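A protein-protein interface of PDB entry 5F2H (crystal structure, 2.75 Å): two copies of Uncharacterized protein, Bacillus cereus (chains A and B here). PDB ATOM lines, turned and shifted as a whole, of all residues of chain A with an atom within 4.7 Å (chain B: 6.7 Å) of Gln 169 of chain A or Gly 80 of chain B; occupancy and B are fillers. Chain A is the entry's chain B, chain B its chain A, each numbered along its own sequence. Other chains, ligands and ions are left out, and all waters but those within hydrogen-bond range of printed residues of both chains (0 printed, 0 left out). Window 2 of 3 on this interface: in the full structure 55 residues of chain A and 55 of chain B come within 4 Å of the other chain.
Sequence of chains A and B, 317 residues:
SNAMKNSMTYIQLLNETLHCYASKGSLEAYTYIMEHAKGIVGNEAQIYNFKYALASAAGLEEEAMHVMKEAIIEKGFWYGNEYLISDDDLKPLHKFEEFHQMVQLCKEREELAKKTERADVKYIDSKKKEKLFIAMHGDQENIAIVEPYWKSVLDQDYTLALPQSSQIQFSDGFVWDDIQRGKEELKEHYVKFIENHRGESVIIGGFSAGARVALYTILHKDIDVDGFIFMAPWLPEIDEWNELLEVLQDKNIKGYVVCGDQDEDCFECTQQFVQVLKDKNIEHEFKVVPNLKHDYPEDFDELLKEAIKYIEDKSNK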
ATOM      1  N   GLN A 140     -25.213   4.246  19.251  1.00  0.00           N
ATOM      2  CA  GLN A 140     -26.406   3.452  19.056  1.00  0.00           C
ATOM      3  C   GLN A 140     -27.666   4.080  19.612  1.00  0.00           C
ATOM      4  O   GLN A 140     -28.617   3.379  19.999  1.00  0.00           O
ATOM      5  CB  GLN A 140     -26.199   2.063  19.643  1.00  0.00           C
ATOM      6  CG  GLN A 140     -25.063   1.342  18.972  1.00  0.00           C
ATOM      7  CD  GLN A 140     -24.926  -0.060  19.481  1.00  0.00           C
ATOM      8  OE1 GLN A 140     -25.101  -1.026  18.739  1.00  0.00           O
ATOM      9  NE2 GLN A 140     -24.754  -0.184  20.770  1.00  0.00           N
ATOM     10  N   GLN A 167     -23.528   9.036  11.124  1.00  0.00           N
ATOM     11  CA  GLN A 167     -22.999   7.672  11.046  1.00  0.00           C
ATOM     12  C   GLN A 167     -24.022   6.662  11.569  1.00  0.00           C
ATOM     13  O   GLN A 167     -24.068   6.358  12.762  1.00  0.00           O
ATOM     14  CB  GLN A 167     -21.689   7.592  11.833  1.00  0.00           C
ATOM     15  CG  GLN A 167     -20.642   8.644  11.442  1.00  0.00           C
ATOM     16  CD  GLN A 167     -19.491   8.719  12.448  1.00  0.00           C
ATOM     17  OE1 GLN A 167     -18.960   7.697  12.895  1.00  0.00           O
ATOM     18  NE2 GLN A 167     -19.113   9.943  12.819  1.00  0.00           N
ATOM     19  N   ILE A 168     -24.787   6.094  10.638  1.00  0.00           N
ATOM     20  CA  ILE A 168     -25.848   5.124  10.948  1.00  0.00           C
ATOM     21  C   ILE A 168     -25.323   3.679  10.954  1.00  0.00           C
ATOM     22  O   ILE A 168     -24.586   3.280  10.067  1.00  0.00           O
ATOM     23  CB  ILE A 168     -27.034   5.305   9.953  1.00  0.00           C
ATOM     24  CG1 ILE A 168     -28.286   4.579  10.432  1.00  0.00           C
ATOM     25  CG2 ILE A 168     -26.654   4.880   8.540  1.00  0.00           C
ATOM     26  CD1 ILE A 168     -29.472   4.777   9.516  1.00  0.00           C
ATOM     27  N   GLN A 169     -25.698   2.914  11.973  1.00  0.00           N
ATOM     28  CA  GLN A 169     -25.271   1.517  12.136  1.00  0.00           C
ATOM     29  C   GLN A 169     -26.408   0.521  11.896  1.00  0.00           C
ATOM     30  O   GLN A 169     -26.164  -0.629  11.585  1.00  0.00           O
ATOM     31  CB  GLN A 169     -24.720   1.342  13.547  1.00  0.00           C
ATOM     32  CG  GLN A 169     -24.202  -0.051  13.869  1.00  0.00           C
ATOM     33  CD  GLN A 169     -23.872  -0.202  15.339  1.00  0.00           C
ATOM     34  OE1 GLN A 169     -23.560   0.779  16.020  1.00  0.00           O
ATOM     35  NE2 GLN A 169     -23.972  -1.428  15.849  1.00  0.00           N
ATOM     36  N   PHE A 170     -27.640   0.967  12.116  1.00  0.00           N
ATOM     37  CA  PHE A 170     -28.860   0.182  11.923  1.00  0.00           C
ATOM     38  C   PHE A 170     -30.038   1.141  12.046  1.00  0.00           C
ATOM     39  O   PHE A 170     -29.857   2.280  12.466  1.00  0.00           O
ATOM     40  CB  PHE A 170     -28.981  -0.952  12.937  1.00  0.00           C
ATOM     41  CG  PHE A 170     -28.966  -0.489  14.347  1.00  0.00           C
ATOM     42  CD1 PHE A 170     -30.150  -0.147  14.988  1.00  0.00           C
ATOM     43  CD2 PHE A 170     -27.760  -0.367  15.035  1.00  0.00           C
ATOM     44  CE1 PHE A 170     -30.128   0.305  16.293  1.00  0.00           C
ATOM     45  CE2 PHE A 170     -27.731   0.085  16.341  1.00  0.00           C
ATOM     46  CZ  PHE A 170     -28.915   0.418  16.973  1.00  0.00           C
ATOM     47  N   GLY A 173     -30.392   3.861  14.736  1.00  0.00           N
ATOM     48  CA  GLY A 173     -29.250   3.761  15.671  1.00  0.00           C
ATOM     49  C   GLY A 173     -28.056   4.506  15.062  1.00  0.00           C
ATOM     50  O   GLY A 173     -27.621   4.183  13.970  1.00  0.00           O
ATOM     51  N   VAL A 175     -23.959   6.411  15.577  1.00  0.00           N
ATOM     52  CA  VAL A 175     -22.691   6.371  16.345  1.00  0.00           C
ATOM     53  C   VAL A 175     -21.680   7.450  16.064  1.00  0.00           C
ATOM     54  O   VAL A 175     -21.668   8.029  14.972  1.00  0.00           O
ATOM     55  CB  VAL A 175     -21.908   5.064  16.103  1.00  0.00           C
ATOM     56  CG1 VAL A 175     -22.711   3.861  16.582  1.00  0.00           C
ATOM     57  CG2 VAL A 175     -21.553   4.906  14.636  1.00  0.00           C
ATOM     58  N   GLN B  46     -33.358  -1.967  17.985  1.00  0.00           N
ATOM     59  CA  GLN B  46     -32.356  -2.426  18.945  1.00  0.00           C
ATOM     60  C   GLN B  46     -32.962  -3.449  19.900  1.00  0.00           C
ATOM     61  O   GLN B  46     -32.283  -4.411  20.291  1.00  0.00           O
ATOM     62  CB  GLN B  46     -31.820  -1.237  19.729  1.00  0.00           C
ATOM     63  CG  GLN B  46     -30.728  -1.537  20.739  1.00  0.00           C
ATOM     64  CD  GLN B  46     -29.452  -2.094  20.125  1.00  0.00           C
ATOM     65  OE1 GLN B  46     -29.481  -3.074  19.381  1.00  0.00           O
ATOM     66  NE2 GLN B  46     -28.306  -1.524  20.523  1.00  0.00           N
ATOM     67  N   TRP B  78     -33.725  -2.621   9.541  1.00  0.00           N
ATOM     68  CA  TRP B  78     -32.602  -3.324   8.912  1.00  0.00           C
ATOM     69  C   TRP B  78     -31.400  -3.284   9.854  1.00  0.00           C
ATOM     70  O   TRP B  78     -31.300  -2.402  10.707  1.00  0.00           O
ATOM     71  CB  TRP B  78     -32.209  -2.689   7.573  1.00  0.00           C
ATOM     72  CG  TRP B  78     -31.630  -1.322   7.715  1.00  0.00           C
ATOM     73  CD1 TRP B  78     -32.293  -0.134   7.637  1.00  0.00           C
ATOM     74  CD2 TRP B  78     -30.267  -1.004   8.002  1.00  0.00           C
ATOM     75  NE1 TRP B  78     -31.419   0.910   7.838  1.00  0.00           N
ATOM     76  CE2 TRP B  78     -30.165   0.401   8.060  1.00  0.00           C
ATOM     77  CE3 TRP B  78     -29.121  -1.772   8.217  1.00  0.00           C
ATOM     78  CZ2 TRP B  78     -28.958   1.052   8.334  1.00  0.00           C
ATOM     79  CZ3 TRP B  78     -27.924  -1.124   8.481  1.00  0.00           C
ATOM     80  CH2 TRP B  78     -27.854   0.272   8.539  1.00  0.00           C
ATOM     81  N   TYR B  79     -30.474  -4.221   9.663  1.00  0.00           N
ATOM     82  CA  TYR B  79     -29.259  -4.307  10.472  1.00  0.00           C
ATOM     83  C   TYR B  79     -28.034  -4.522   9.575  1.00  0.00           C
ATOM     84  O   TYR B  79     -28.166  -4.928   8.423  1.00  0.00           O
ATOM     85  CB  TYR B  79     -29.378  -5.438  11.492  1.00  0.00           C
ATOM     86  CG  TYR B  79     -30.588  -5.311  12.378  1.00  0.00           C
ATOM     87  CD1 TYR B  79     -30.551  -4.563  13.546  1.00  0.00           C
ATOM     88  CD2 TYR B  79     -31.794  -5.919  12.029  1.00  0.00           C
ATOM     89  CE1 TYR B  79     -31.675  -4.435  14.352  1.00  0.00           C
ATOM     90  CE2 TYR B  79     -32.909  -5.811  12.834  1.00  0.00           C
ATOM     91  CZ  TYR B  79     -32.850  -5.068  13.996  1.00  0.00           C
ATOM     92  OH  TYR B  79     -33.976  -4.942  14.789  1.00  0.00           O
ATOM     93  N   GLY B  80     -26.847  -4.248  10.119  1.00  0.00           N
ATOM     94  CA  GLY B  80     -25.583  -4.397   9.388  1.00  0.00           C
ATOM     95  C   GLY B  80     -25.406  -5.738   8.697  1.00  0.00           C
ATOM     96  O   GLY B  80     -25.700  -6.796   9.258  1.00  0.00           O
ATOM     97  N   ASN B  81     -24.891  -5.695   7.475  1.00  0.00           N
ATOM     98  CA  ASN B  81     -24.691  -6.902   6.713  1.00  0.00           C
ATOM     99  C   ASN B  81     -23.649  -7.749   7.392  1.00  0.00           C
ATOM    100  O   ASN B  81     -23.869  -8.937   7.612  1.00  0.00           O
ATOM    101  CB  ASN B  81     -24.203  -6.580   5.302  1.00  0.00           C
ATOM    102  CG  ASN B  81     -23.902  -7.827   4.495  1.00  0.00           C
ATOM    103  OD1 ASN B  81     -24.537  -8.862   4.659  1.00  0.00           O
ATOM    104  ND2 ASN B  81     -22.932  -7.730   3.617  1.00  0.00           N
ATOM    105  N   GLU B  82     -22.514  -7.134   7.723  1.00  0.00           N
ATOM    106  CA  GLU B  82     -21.424  -7.862   8.365  1.00  0.00           C
ATOM    107  C   GLU B  82     -21.923  -8.500   9.658  1.00  0.00           C
ATOM    108  O   GLU B  82     -21.697  -9.684   9.906  1.00  0.00           O
ATOM    109  CB  GLU B  82     -20.229  -6.955   8.602  1.00  0.00           C
ATOM    110  CG  GLU B  82     -18.981  -7.695   9.043  1.00  0.00           C
ATOM    111  CD  GLU B  82     -17.782  -6.759   9.120  1.00  0.00           C
ATOM    112  OE1 GLU B  82     -16.650  -7.225   9.413  1.00  0.00           O
ATOM    113  OE2 GLU B  82     -17.974  -5.542   8.886  1.00  0.00           O
ATOM    114  N   TYR B  83     -22.594  -7.721  10.492  1.00  0.00           N
ATOM    115  CA  TYR B  83     -23.136  -8.285  11.700  1.00  0.00           C
ATOM    116  C   TYR B  83     -23.991  -9.498  11.367  1.00  0.00           C
ATOM    117  O   TYR B  83     -23.747 -10.605  11.869  1.00  0.00           O
ATOM    118  CB  TYR B  83     -23.976  -7.257  12.430  1.00  0.00           C
ATOM    119  CG  TYR B  83     -24.877  -7.865  13.463  1.00  0.00           C
ATOM    120  CD1 TYR B  83     -24.377  -8.273  14.701  1.00  0.00           C
ATOM    121  CD2 TYR B  83     -26.246  -8.007  13.214  1.00  0.00           C
ATOM    122  CE1 TYR B  83     -25.209  -8.814  15.662  1.00  0.00           C
ATOM    123  CE2 TYR B  83     -27.091  -8.552  14.174  1.00  0.00           C
ATOM    124  CZ  TYR B  83     -26.570  -8.948  15.397  1.00  0.00           C
ATOM    125  OH  TYR B  83     -27.381  -9.490  16.351  1.00  0.00           O
ATOM    126  N   LEU B  84     -24.993  -9.286  10.513  1.00  0.00           N
ATOM    127  CA  LEU B  84     -25.881 -10.365  10.116  1.00  0.00           C
ATOM    128  C   LEU B  84     -25.181 -11.649   9.711  1.00  0.00           C
ATOM    129  O   LEU B  84     -25.456 -12.712  10.297  1.00  0.00           O
ATOM    130  CB  LEU B  84     -26.837  -9.926   9.004  1.00  0.00           C
ATOM    131  CG  LEU B  84     -27.948  -8.980   9.458  1.00  0.00           C
ATOM    132  CD1 LEU B  84     -28.707  -8.429   8.269  1.00  0.00           C
ATOM    133  CD2 LEU B  84     -28.881  -9.688  10.447  1.00  0.00           C
ATOM    134  N   ILE B  85     -24.266 -11.561   8.745  1.00  0.00           N
ATOM    135  CA  ILE B  85     -23.576 -12.768   8.295  1.00  0.00           C
ATOM    136  C   ILE B  85     -22.366 -13.170   9.138  1.00  0.00           C
ATOM    137  O   ILE B  85     -21.678 -14.116   8.781  1.00  0.00           O
ATOM    138  CB  ILE B  85     -23.171 -12.697   6.801  1.00  0.00           C
ATOM    139  CG1 ILE B  85     -21.973 -11.763   6.571  1.00  0.00           C
ATOM    140  CG2 ILE B  85     -24.386 -12.320   5.949  1.00  0.00           C
ATOM    141  CD1 ILE B  85     -21.492 -11.743   5.139  1.00  0.00           C
ATOM    142  N   CYS B 106     -32.228  -6.635   4.230  1.00  0.00           N
ATOM    143  CA  CYS B 106     -31.458  -5.646   5.001  1.00  0.00           C
ATOM    144  C   CYS B 106     -30.329  -5.016   4.190  1.00  0.00           C
ATOM    145  O   CYS B 106     -30.088  -3.818   4.297  1.00  0.00           O
ATOM    146  CB  CYS B 106     -30.852  -6.258   6.266  1.00  0.00           C
ATOM    147  SG  CYS B 106     -32.043  -6.759   7.535  1.00  0.00           S
ATOM    148  N   GLU B 110     -29.761  -1.186   3.772  1.00  0.00           N
ATOM    149  CA  GLU B 110     -28.496  -0.674   4.287  1.00  0.00           C
ATOM    150  C   GLU B 110     -27.758   0.134   3.239  1.00  0.00           C
ATOM    151  O   GLU B 110     -27.322   1.245   3.519  1.00  0.00           O
ATOM    152  CB  GLU B 110     -27.602  -1.828   4.736  1.00  0.00           C
ATOM    153  CG  GLU B 110     -26.238  -1.462   5.326  1.00  0.00           C
ATOM    154  CD  GLU B 110     -25.468  -2.725   5.714  1.00  0.00           C
ATOM    155  OE1 GLU B 110     -26.104  -3.803   5.662  1.00  0.00           O
ATOM    156  OE2 GLU B 110     -24.265  -2.676   6.086  1.00  0.00           O
ATOM    157  N   LYS B 114     -26.953   3.990   3.909  1.00  0.00           N
ATOM    158  CA  LYS B 114     -25.600   4.442   4.110  1.00  0.00           C
ATOM    159  C   LYS B 114     -25.167   5.491   3.092  1.00  0.00           C
ATOM    160  O   LYS B 114     -24.457   6.438   3.450  1.00  0.00           O
ATOM    161  CB  LYS B 114     -24.718   3.211   4.240  1.00  0.00           C
ATOM    162  CG  LYS B 114     -23.310   3.451   4.738  1.00  0.00           C
ATOM    163  CD  LYS B 114     -22.776   2.179   5.402  1.00  0.00           C
ATOM    164  CE  LYS B 114     -23.470   1.936   6.747  1.00  0.00           C
ATOM    165  NZ  LYS B 114     -23.034   0.681   7.427  1.00  0.00           N
ATOM    166  N   GLU B 117     -26.592   8.806   4.440  1.00  0.00           N
ATOM    167  CA  GLU B 117     -26.259   9.363   5.751  1.00  0.00           C
ATOM    168  C   GLU B 117     -26.334  10.887   5.684  1.00  0.00           C
ATOM    169  O   GLU B 117     -26.039  11.476   4.647  1.00  0.00           O
ATOM    170  CB  GLU B 117     -24.857   8.925   6.211  1.00  0.00           C
ATOM    171  CG  GLU B 117     -24.714   7.439   6.533  1.00  0.00           C
ATOM    172  CD  GLU B 117     -23.336   7.057   7.089  1.00  0.00           C
ATOM    173  OE1 GLU B 117     -22.389   7.876   7.012  1.00  0.00           O
ATOM    174  OE2 GLU B 117     -23.193   5.920   7.610  1.00  0.00           O
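N of Ile 168 of chain A sits at hydrogen-bond distance from OE2 of Glu 117 of chain B, at 3.4 Å.
Printed residues of chain B within 4 Å of Gln 140 of chain A: Gln 46 (3.7 Å). Gln 169 of chain A touches just these residues of chain B: Trp 78 and Gly 80. Of the printed residues of chain A, Gln 46 of chain B touches Gln 140. Of the printed residues of chain A, Trp 78 of chain B touches Ile 168, Gln 169 and Phe 170. Of the printed residues of chain A, Tyr 79 of chain B touches Phe 170 (3.98 Å). Gly 80 of chain B touches one residue of chain A. The nearest residue of chain B that does not touch Gln 169 of chain A is Tyr 79 of chain B (4.8 Å). The nearest printed residue of chain A that does not touch Gly 80 of chain B is Phe 170 of chain A (4.8 Å).
Of the 7 printed residues of chain A, 5 touch a printed residue of chain B. Hydrophobic or aromatic side chains of chain A within 4 Å of the printed part of chain B: Ile 168 and Phe 170. Of the 13 printed residues of chain B, 6 touch a printed residue of chain A. Among the printed residues, 9 pairs touch across the chains. Among the printed residues, no Asp or Glu carboxylate lies within 4 Å of a Lys or Arg side-chain nitrogen of the other chain.
Among the printed residues, pairs that only touch across the chains: Phe 170 of chain A with Trp 78 of chain B, Gln 169 of chain A with Trp 78 of chain B, Gln 140 of chain A with Gln 46 of chain B, Ile 168 of chain A with Lys 114 of chain B, Gln 167 of chain A with Glu 117 of chain B, Ile 168 of chain A with Trp 78 of chain B, Gln 169 of chain A with Gly 80 of chain B and Phe 170 of chain A with Tyr 79 of chain B.
No position is printed for both chains. Of the 9 pairs that touch across the chains among the printed residues, none has its exchanged pair printed and touching as well.
The side-chain sulfur (SG) of Cys 106 of chain B sits at hydrogen-bond distance from the backbone NH (N) of Tyr 79 of chain B, at 3.7 Å. NZ of Lys 114 of chain B is in salt-bridge range of OE2 of Glu 110 of chain B (3.8 Å). The side-chain amide oxygen of Gln 140 of chain A sits at hydrogen-bond distance from the side-chain amide nitrogen of Gln 169 of chain A (3.1 Å). O of Gln 167 of chain A is in hydrogen-bond range of N of Val 175 of chain A.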
